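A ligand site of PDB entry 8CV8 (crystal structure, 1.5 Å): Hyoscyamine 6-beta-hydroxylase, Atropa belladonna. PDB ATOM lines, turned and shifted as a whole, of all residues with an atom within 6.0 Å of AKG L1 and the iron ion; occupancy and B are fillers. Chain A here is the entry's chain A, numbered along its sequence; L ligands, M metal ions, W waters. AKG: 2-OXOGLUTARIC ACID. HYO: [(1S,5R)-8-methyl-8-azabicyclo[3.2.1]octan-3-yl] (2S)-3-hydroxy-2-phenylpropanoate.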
ATOM      1  N   LYS A 129     -27.370  -0.774 -17.476  1.00  0.00           N
ATOM      2  CA  LYS A 129     -25.936  -0.970 -17.151  1.00  0.00           C
ATOM      3  C   LYS A 129     -25.311   0.378 -16.776  1.00  0.00           C
ATOM      4  O   LYS A 129     -25.604   1.388 -17.445  1.00  0.00           O
ATOM      5  CB  LYS A 129     -25.237  -1.564 -18.382  1.00  0.00           C
ATOM      6  CG  LYS A 129     -23.718  -1.615 -18.347  1.00  0.00           C
ATOM      7  CD  LYS A 129     -23.153  -2.441 -19.487  1.00  0.00           C
ATOM      8  CE  LYS A 129     -23.155  -1.725 -20.818  1.00  0.00           C
ATOM      9  NZ  LYS A 129     -22.109  -0.684 -20.895  1.00  0.00           N
ATOM     10  N   LEU A 198     -13.248  -2.373 -18.190  1.00  0.00           N
ATOM     11  CA  LEU A 198     -14.674  -1.996 -18.066  1.00  0.00           C
ATOM     12  C   LEU A 198     -15.260  -2.811 -16.924  1.00  0.00           C
ATOM     13  O   LEU A 198     -15.346  -4.042 -17.056  1.00  0.00           O
ATOM     14  CB  LEU A 198     -15.380  -2.278 -19.398  1.00  0.00           C
ATOM     15  CG  LEU A 198     -15.293  -1.175 -20.452  1.00  0.00           C
ATOM     16  CD1 LEU A 198     -13.861  -0.917 -20.887  1.00  0.00           C
ATOM     17  CD2 LEU A 198     -16.164  -1.525 -21.647  1.00  0.00           C
ATOM     18  N   ASN A 200     -18.579  -3.503 -15.188  1.00  0.00           N
ATOM     19  CA  ASN A 200     -20.003  -3.382 -15.585  1.00  0.00           C
ATOM     20  C   ASN A 200     -20.879  -3.705 -14.385  1.00  0.00           C
ATOM     21  O   ASN A 200     -20.673  -4.756 -13.777  1.00  0.00           O
ATOM     22  CB  ASN A 200     -20.354  -4.330 -16.727  1.00  0.00           C
ATOM     23  CG  ASN A 200     -19.466  -4.095 -17.922  1.00  0.00           C
ATOM     24  OD1 ASN A 200     -19.371  -2.978 -18.421  1.00  0.00           O
ATOM     25  ND2 ASN A 200     -18.785  -5.143 -18.369  1.00  0.00           N
ATOM     26  N   TYR A 202     -24.835  -4.187 -13.355  1.00  0.00           N
ATOM     27  CA  TYR A 202     -26.222  -4.484 -13.802  1.00  0.00           C
ATOM     28  C   TYR A 202     -27.120  -4.506 -12.570  1.00  0.00           C
ATOM     29  O   TYR A 202     -27.181  -5.523 -11.875  1.00  0.00           O
ATOM     30  CB  TYR A 202     -26.242  -5.811 -14.558  1.00  0.00           C
ATOM     31  CG  TYR A 202     -25.235  -5.900 -15.673  1.00  0.00           C
ATOM     32  CD1 TYR A 202     -25.514  -5.392 -16.934  1.00  0.00           C
ATOM     33  CD2 TYR A 202     -23.999  -6.476 -15.466  1.00  0.00           C
ATOM     34  CE1 TYR A 202     -24.597  -5.483 -17.963  1.00  0.00           C
ATOM     35  CE2 TYR A 202     -23.067  -6.564 -16.488  1.00  0.00           C
ATOM     36  CZ  TYR A 202     -23.366  -6.076 -17.739  1.00  0.00           C
ATOM     37  OH  TYR A 202     -22.432  -6.171 -18.737  1.00  0.00           O
ATOM     38  N   SER A 214     -26.790  -5.581 -21.780  1.00  0.00           N
ATOM     39  CA  SER A 214     -25.821  -5.269 -22.850  1.00  0.00           C
ATOM     40  C   SER A 214     -26.370  -5.845 -24.151  1.00  0.00           C
ATOM     41  O   SER A 214     -26.616  -7.062 -24.193  1.00  0.00           O
ATOM     42  CB  SER A 214     -24.461  -5.823 -22.507  1.00  0.00           C
ATOM     43  OG  SER A 214     -23.427  -5.178 -23.238  1.00  0.00           O
ATOM     44  N   HIS A 217     -23.396  -7.911 -29.378  1.00  0.00           N
ATOM     45  CA  HIS A 217     -22.225  -7.235 -29.988  1.00  0.00           C
ATOM     46  C   HIS A 217     -21.060  -8.200 -30.091  1.00  0.00           C
ATOM     47  O   HIS A 217     -20.928  -9.095 -29.248  1.00  0.00           O
ATOM     48  CB  HIS A 217     -21.833  -5.982 -29.193  1.00  0.00           C
ATOM     49  CG  HIS A 217     -21.306  -6.275 -27.822  1.00  0.00           C
ATOM     50  ND1 HIS A 217     -22.131  -6.649 -26.781  1.00  0.00           N
ATOM     51  CD2 HIS A 217     -20.052  -6.275 -27.326  1.00  0.00           C
ATOM     52  CE1 HIS A 217     -21.400  -6.865 -25.704  1.00  0.00           C
ATOM     53  NE2 HIS A 217     -20.117  -6.631 -26.007  1.00  0.00           N
ATOM     54  N   TYR A 218     -20.183  -7.964 -31.072  1.00  0.00           N
ATOM     55  CA  TYR A 218     -18.749  -8.287 -30.960  1.00  0.00           C
ATOM     56  C   TYR A 218     -18.086  -7.210 -30.111  1.00  0.00           C
ATOM     57  O   TYR A 218     -18.477  -6.032 -30.208  1.00  0.00           O
ATOM     58  CB  TYR A 218     -18.027  -8.206 -32.306  1.00  0.00           C
ATOM     59  CG  TYR A 218     -18.414  -9.191 -33.379  1.00  0.00           C
ATOM     60  CD1 TYR A 218     -17.891 -10.474 -33.403  1.00  0.00           C
ATOM     61  CD2 TYR A 218     -19.233  -8.799 -34.417  1.00  0.00           C
ATOM     62  CE1 TYR A 218     -18.218 -11.360 -34.420  1.00  0.00           C
ATOM     63  CE2 TYR A 218     -19.567  -9.677 -35.435  1.00  0.00           C
ATOM     64  CZ  TYR A 218     -19.049 -10.961 -35.437  1.00  0.00           C
ATOM     65  OH  TYR A 218     -19.382 -11.823 -36.451  1.00  0.00           O
ATOM     66  N   ASP A 219     -17.056  -7.572 -29.354  1.00  0.00           N
ATOM     67  CA  ASP A 219     -16.066  -6.591 -28.854  1.00  0.00           C
ATOM     68  C   ASP A 219     -15.253  -6.149 -30.073  1.00  0.00           C
ATOM     69  O   ASP A 219     -14.802  -7.017 -30.836  1.00  0.00           O
ATOM     70  CB  ASP A 219     -15.202  -7.181 -27.737  1.00  0.00           C
ATOM     71  CG  ASP A 219     -15.951  -7.470 -26.437  1.00  0.00           C
ATOM     72  OD1 ASP A 219     -17.136  -7.112 -26.327  1.00  0.00           O
ATOM     73  OD2 ASP A 219     -15.341  -8.074 -25.548  1.00  0.00           O
ATOM     74  N   THR A 224     -10.675 -10.043 -25.456  1.00  0.00           N
ATOM     75  CA  THR A 224     -11.228  -9.589 -24.156  1.00  0.00           C
ATOM     76  C   THR A 224     -11.183 -10.761 -23.181  1.00  0.00           C
ATOM     77  O   THR A 224     -11.554 -11.888 -23.585  1.00  0.00           O
ATOM     78  CB  THR A 224     -12.674  -9.084 -24.303  1.00  0.00           C
ATOM     79  OG1 THR A 224     -12.656  -7.980 -25.212  1.00  0.00           O
ATOM     80  CG2 THR A 224     -13.260  -8.673 -22.974  1.00  0.00           C
ATOM     81  N   LEU A 226     -12.963 -11.733 -19.582  1.00  0.00           N
ATOM     82  CA  LEU A 226     -14.164 -11.321 -18.821  1.00  0.00           C
ATOM     83  C   LEU A 226     -14.201 -12.171 -17.537  1.00  0.00           C
ATOM     84  O   LEU A 226     -14.118 -13.396 -17.629  1.00  0.00           O
ATOM     85  CB  LEU A 226     -15.393 -11.515 -19.713  1.00  0.00           C
ATOM     86  CG  LEU A 226     -16.769 -11.161 -19.154  1.00  0.00           C
ATOM     87  CD1 LEU A 226     -17.251 -12.162 -18.104  1.00  0.00           C
ATOM     88  CD2 LEU A 226     -16.820  -9.746 -18.609  1.00  0.00           C
ATOM     89  N   GLN A 228     -16.587 -13.062 -14.279  1.00  0.00           N
ATOM     90  CA  GLN A 228     -17.992 -13.028 -13.815  1.00  0.00           C
ATOM     91  C   GLN A 228     -18.182 -14.051 -12.699  1.00  0.00           C
ATOM     92  O   GLN A 228     -17.470 -15.069 -12.705  1.00  0.00           O
ATOM     93  CB  GLN A 228     -18.955 -13.305 -14.968  1.00  0.00           C
ATOM     94  CG  GLN A 228     -18.693 -14.627 -15.687  1.00  0.00           C
ATOM     95  CD  GLN A 228     -19.830 -15.072 -16.573  1.00  0.00           C
ATOM     96  OE1 GLN A 228     -20.866 -14.416 -16.673  1.00  0.00           O
ATOM     97  NE2 GLN A 228     -19.646 -16.189 -17.232  1.00  0.00           N
ATOM     98  N   GLY A 232     -25.931 -14.320 -16.651  1.00  0.00           N
ATOM     99  CA  GLY A 232     -26.431 -13.167 -17.425  1.00  0.00           C
ATOM    100  C   GLY A 232     -25.788 -13.068 -18.787  1.00  0.00           C
ATOM    101  O   GLY A 232     -26.415 -12.500 -19.694  1.00  0.00           O
ATOM    102  N   LEU A 233     -24.554 -13.585 -18.926  1.00  0.00           N
ATOM    103  CA  LEU A 233     -23.819 -13.535 -20.211  1.00  0.00           C
ATOM    104  C   LEU A 233     -24.377 -14.621 -21.134  1.00  0.00           C
ATOM    105  O   LEU A 233     -24.506 -15.783 -20.680  1.00  0.00           O
ATOM    106  CB  LEU A 233     -22.328 -13.731 -19.956  1.00  0.00           C
ATOM    107  CG  LEU A 233     -21.442 -13.752 -21.206  1.00  0.00           C
ATOM    108  CD1 LEU A 233     -21.497 -12.432 -21.952  1.00  0.00           C
ATOM    109  CD2 LEU A 233     -20.020 -14.106 -20.818  1.00  0.00           C
ATOM    110  N   ASN A 255     -13.225 -13.726 -25.035  1.00  0.00           N
ATOM    111  CA  ASN A 255     -14.044 -13.301 -26.199  1.00  0.00           C
ATOM    112  C   ASN A 255     -13.093 -12.810 -27.293  1.00  0.00           C
ATOM    113  O   ASN A 255     -12.368 -11.830 -27.046  1.00  0.00           O
ATOM    114  CB  ASN A 255     -15.017 -12.176 -25.834  1.00  0.00           C
ATOM    115  CG  ASN A 255     -16.247 -12.624 -25.068  1.00  0.00           C
ATOM    116  OD1 ASN A 255     -16.883 -13.605 -25.411  1.00  0.00           O
ATOM    117  ND2 ASN A 255     -16.622 -11.873 -24.045  1.00  0.00           N
ATOM    118  N   HIS A 273     -22.048 -11.655 -28.259  1.00  0.00           N
ATOM    119  CA  HIS A 273     -22.560 -11.922 -26.891  1.00  0.00           C
ATOM    120  C   HIS A 273     -23.428 -10.757 -26.425  1.00  0.00           C
ATOM    121  O   HIS A 273     -23.325  -9.655 -26.973  1.00  0.00           O
ATOM    122  CB  HIS A 273     -21.405 -12.221 -25.937  1.00  0.00           C
ATOM    123  CG  HIS A 273     -20.356 -11.159 -25.926  1.00  0.00           C
ATOM    124  ND1 HIS A 273     -19.329 -11.130 -26.838  1.00  0.00           N
ATOM    125  CD2 HIS A 273     -20.167 -10.093 -25.108  1.00  0.00           C
ATOM    126  CE1 HIS A 273     -18.558 -10.088 -26.584  1.00  0.00           C
ATOM    127  NE2 HIS A 273     -19.041  -9.454 -25.531  1.00  0.00           N
ATOM    128  N   ARG A 274     -24.246 -11.030 -25.418  1.00  0.00           N
ATOM    129  CA  ARG A 274     -25.158 -10.038 -24.796  1.00  0.00           C
ATOM    130  C   ARG A 274     -25.266 -10.360 -23.303  1.00  0.00           C
ATOM    131  O   ARG A 274     -24.827 -11.455 -22.879  1.00  0.00           O
ATOM    132  CB  ARG A 274     -26.532 -10.062 -25.460  1.00  0.00           C
ATOM    133  CG  ARG A 274     -27.390 -11.255 -25.072  1.00  0.00           C
ATOM    134  CD  ARG A 274     -28.717 -11.289 -25.813  1.00  0.00           C
ATOM    135  NE  ARG A 274     -29.492 -12.435 -25.397  1.00  0.00           N
ATOM    136  CZ  ARG A 274     -30.615 -12.851 -25.988  1.00  0.00           C
ATOM    137  NH1 ARG A 274     -31.092 -12.202 -27.036  1.00  0.00           N
ATOM    138  NH2 ARG A 274     -31.240 -13.924 -25.531  1.00  0.00           N
ATOM    139  N   VAL A 275     -25.838  -9.444 -22.551  1.00  0.00           N
ATOM    140  CA  VAL A 275     -26.110  -9.639 -21.099  1.00  0.00           C
ATOM    141  C   VAL A 275     -27.581  -9.340 -20.849  1.00  0.00           C
ATOM    142  O   VAL A 275     -28.060  -8.267 -21.250  1.00  0.00           O
ATOM    143  CB  VAL A 275     -25.200  -8.778 -20.212  1.00  0.00           C
ATOM    144  CG1 VAL A 275     -25.522  -9.005 -18.743  1.00  0.00           C
ATOM    145  CG2 VAL A 275     -23.734  -9.059 -20.499  1.00  0.00           C
ATOM    146  N   ARG A 283     -25.457  -7.582 -10.532  1.00  0.00           N
ATOM    147  CA  ARG A 283     -24.357  -8.378 -11.125  1.00  0.00           C
ATOM    148  C   ARG A 283     -23.237  -7.400 -11.466  1.00  0.00           C
ATOM    149  O   ARG A 283     -23.526  -6.318 -12.000  1.00  0.00           O
ATOM    150  CB  ARG A 283     -24.834  -9.115 -12.372  1.00  0.00           C
ATOM    151  CG  ARG A 283     -23.737  -9.847 -13.133  1.00  0.00           C
ATOM    152  CD  ARG A 283     -24.340 -10.747 -14.195  1.00  0.00           C
ATOM    153  NE  ARG A 283     -23.327 -11.463 -14.951  1.00  0.00           N
ATOM    154  CZ  ARG A 283     -22.631 -10.972 -15.970  1.00  0.00           C
ATOM    155  NH1 ARG A 283     -22.829  -9.732 -16.386  1.00  0.00           N
ATOM    156  NH2 ARG A 283     -21.745 -11.730 -16.580  1.00  0.00           N
ATOM    157  N   SER A 285     -19.501  -7.472 -13.549  1.00  0.00           N
ATOM    158  CA  SER A 285     -18.520  -8.194 -14.394  1.00  0.00           C
ATOM    159  C   SER A 285     -17.327  -7.268 -14.643  1.00  0.00           C
ATOM    160  O   SER A 285     -17.484  -6.036 -14.576  1.00  0.00           O
ATOM    161  CB  SER A 285     -19.121  -8.678 -15.685  1.00  0.00           C
ATOM    162  OG  SER A 285     -19.413  -7.607 -16.554  1.00  0.00           O
ATOM    163  N   ALA A 287     -14.486  -6.689 -17.510  1.00  0.00           N
ATOM    164  CA  ALA A 287     -14.043  -6.939 -18.893  1.00  0.00           C
ATOM    165  C   ALA A 287     -12.727  -6.202 -19.129  1.00  0.00           C
ATOM    166  O   ALA A 287     -12.699  -4.976 -18.945  1.00  0.00           O
ATOM    167  CB  ALA A 287     -15.102  -6.490 -19.866  1.00  0.00           C
ATOM    168  N   LEU A 289     -10.473  -5.307 -22.118  1.00  0.00           N
ATOM    169  CA  LEU A 289     -10.527  -5.216 -23.590  1.00  0.00           C
ATOM    170  C   LEU A 289      -9.151  -4.781 -24.075  1.00  0.00           C
ATOM    171  O   LEU A 289      -8.796  -3.611 -23.883  1.00  0.00           O
ATOM    172  CB  LEU A 289     -11.601  -4.214 -23.998  1.00  0.00           C
ATOM    173  CG  LEU A 289     -13.033  -4.735 -23.965  1.00  0.00           C
ATOM    174  CD1 LEU A 289     -13.542  -4.900 -22.534  1.00  0.00           C
ATOM    175  CD2 LEU A 289     -13.940  -3.809 -24.751  1.00  0.00           C
HETATM  176  C1  AKG L   1     -18.513  -6.059 -22.374  1.00  0.00           C
HETATM  177  O1  AKG L   1     -18.095  -5.931 -23.527  1.00  0.00           O
HETATM  178  O2  AKG L   1     -18.289  -5.217 -21.489  1.00  0.00           O
HETATM  179  C2  AKG L   1     -19.193  -7.146 -22.075  1.00  0.00           C
HETATM  180  O5  AKG L   1     -19.519  -7.900 -23.007  1.00  0.00           O
HETATM  181  C3  AKG L   1     -19.520  -7.562 -20.661  1.00  0.00           C
HETATM  182  C4  AKG L   1     -20.257  -8.885 -20.543  1.00  0.00           C
HETATM  183  C5  AKG L   1     -20.672  -9.307 -19.148  1.00  0.00           C
HETATM  184  O3  AKG L   1     -20.616 -10.514 -18.861  1.00  0.00           O
HETATM  185  O4  AKG L   1     -21.090  -8.428 -18.351  1.00  0.00           O
HETATM  186  C10 HYO L   2     -18.077  -0.395 -24.952  1.00  0.00           C
HETATM  187  C13 HYO L   2     -15.377   0.002 -26.536  1.00  0.00           C
HETATM  188  C15 HYO L   2     -13.706  -0.261 -28.315  1.00  0.00           C
HETATM  189  C17 HYO L   2     -13.798   1.041 -28.818  1.00  0.00           C
HETATM  190  C20 HYO L   2     -12.936  -1.020 -30.476  1.00  0.00           C
HETATM  191  C21 HYO L   2     -13.035   0.274 -30.975  1.00  0.00           C
HETATM  192  C05 HYO L   2     -19.018  -2.650 -26.434  1.00  0.00           C
HETATM  193  C06 HYO L   2     -18.468  -1.776 -24.415  1.00  0.00           C
HETATM  194  C07 HYO L   2     -17.772  -3.449 -26.018  1.00  0.00           C
HETATM  195  C08 HYO L   2     -17.387  -2.828 -24.669  1.00  0.00           C
HETATM  196  C09 HYO L   2     -18.693  -1.367 -27.206  1.00  0.00           C
HETATM  197  C11 HYO L   2     -17.775  -0.424 -26.452  1.00  0.00           C
HETATM  198  C12 HYO L   2     -20.353  -3.344 -24.538  1.00  0.00           C
HETATM  199  C14 HYO L   2     -14.042  -0.583 -26.888  1.00  0.00           C
HETATM  200  C16 HYO L   2     -12.965  -0.084 -25.926  1.00  0.00           C
HETATM  201  C18 HYO L   2     -13.275  -1.279 -29.153  1.00  0.00           C
HETATM  202  C19 HYO L   2     -13.473   1.297 -30.148  1.00  0.00           C
HETATM  203  N04 HYO L   2     -19.634  -2.226 -25.180  1.00  0.00           N
HETATM  204  O01 HYO L   2     -16.457  -0.915 -26.674  1.00  0.00           O
HETATM  205  O02 HYO L   2     -15.563   1.137 -26.147  1.00  0.00           O
HETATM  206  O03 HYO L   2     -11.704  -0.691 -26.230  1.00  0.00           O
HETATM  207 FE    FE M   1     -18.500  -7.497 -24.834  1.00  0.00          FE
HETATM  208  O   HOH W   1     -16.777  -8.815 -23.591  1.00  0.00           O
HETATM  209  O   HOH W   2     -19.585  -2.737 -21.180  1.00  0.00           O
HETATM  210  O   HOH W   3     -21.647  -4.878 -21.191  1.00  0.00           O
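The side-chain hydroxyl of Ser 285 sits at hydrogen-bond distance from an oxygen (O4) of AKG L1 (2.6 Å). An oxygen (O4) of AKG L1 is in hydrogen-bond range of the side-chain hydroxyl (OH) of Tyr 202, 2.7 Å away. The guanidinium group (NH2) of Arg 283 lies within salt-bridge range of an oxygen (O3) of AKG L1 (2.8 Å). The side-chain amide nitrogen (ND2) of Asn 200 is in hydrogen-bond range of an oxygen (O2) of AKG L1 (3.2 Å).
OD2 of Asp 219 sits at hydrogen-bond distance from OG1 of Thr 224. The backbone carbonyl oxygen of Ser 285 is in hydrogen-bond range of the backbone NH of Asn 200 (2.8 Å). The backbone NH of Tyr 202 lies within hydrogen-bond range of the backbone carbonyl oxygen of Arg 283 (2.8 Å). The side-chain amide oxygen (OE1) of Gln 228 lies within hydrogen-bond range of the guanidinium group (NH2) of Arg 283 (2.8 Å). The backbone NH of Val 275 sits at hydrogen-bond distance from the backbone carbonyl oxygen of Ser 214, 3.0 Å away. N of Leu 198 lies within hydrogen-bond range of O of Ala 287, 2.8 Å away.
Residues that only touch AKG L1: Val 275, Leu 233, Ala 287 and Leu 226. Hydrophobic or aromatic side chains within 4 Å of AKG L1: Tyr 202, His 217, Leu 226, Leu 233, His 273, Val 275 and Ala 287. Within 4 Å of AKG L1: Asn 200, Tyr 202, His 217, Asp 219, Leu 226, Leu 233, His 273, Val 275, Arg 283, Ser 285 and Ala 287. The nearest printed residue that does not touch AKG L1 is Leu 198 (4.3 Å).
The iron ion is bound by OD1 of Asp 219 (2.1 Å), O1 of AKG L1 (2.1 Å), O5 of AKG L1 (2.1 Å), NE2 of His 273 (2.1 Å), NE2 of His 217 (2.2 Å) and water W1 (2.5 Å).
Water W1 bridges OD2 of Asp 219 and ND2 of Asn 255. Water W2 lies within hydrogen-bond range of OD1 of Asn 200 (2.8 Å), O2 of AKG L1 (2.8 Å) and NZ of Lys 129 (3.3 Å). Water W3 lies within hydrogen-bond range of OG of Ser 214, OH of Tyr 202 and O2 of AKG L1.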
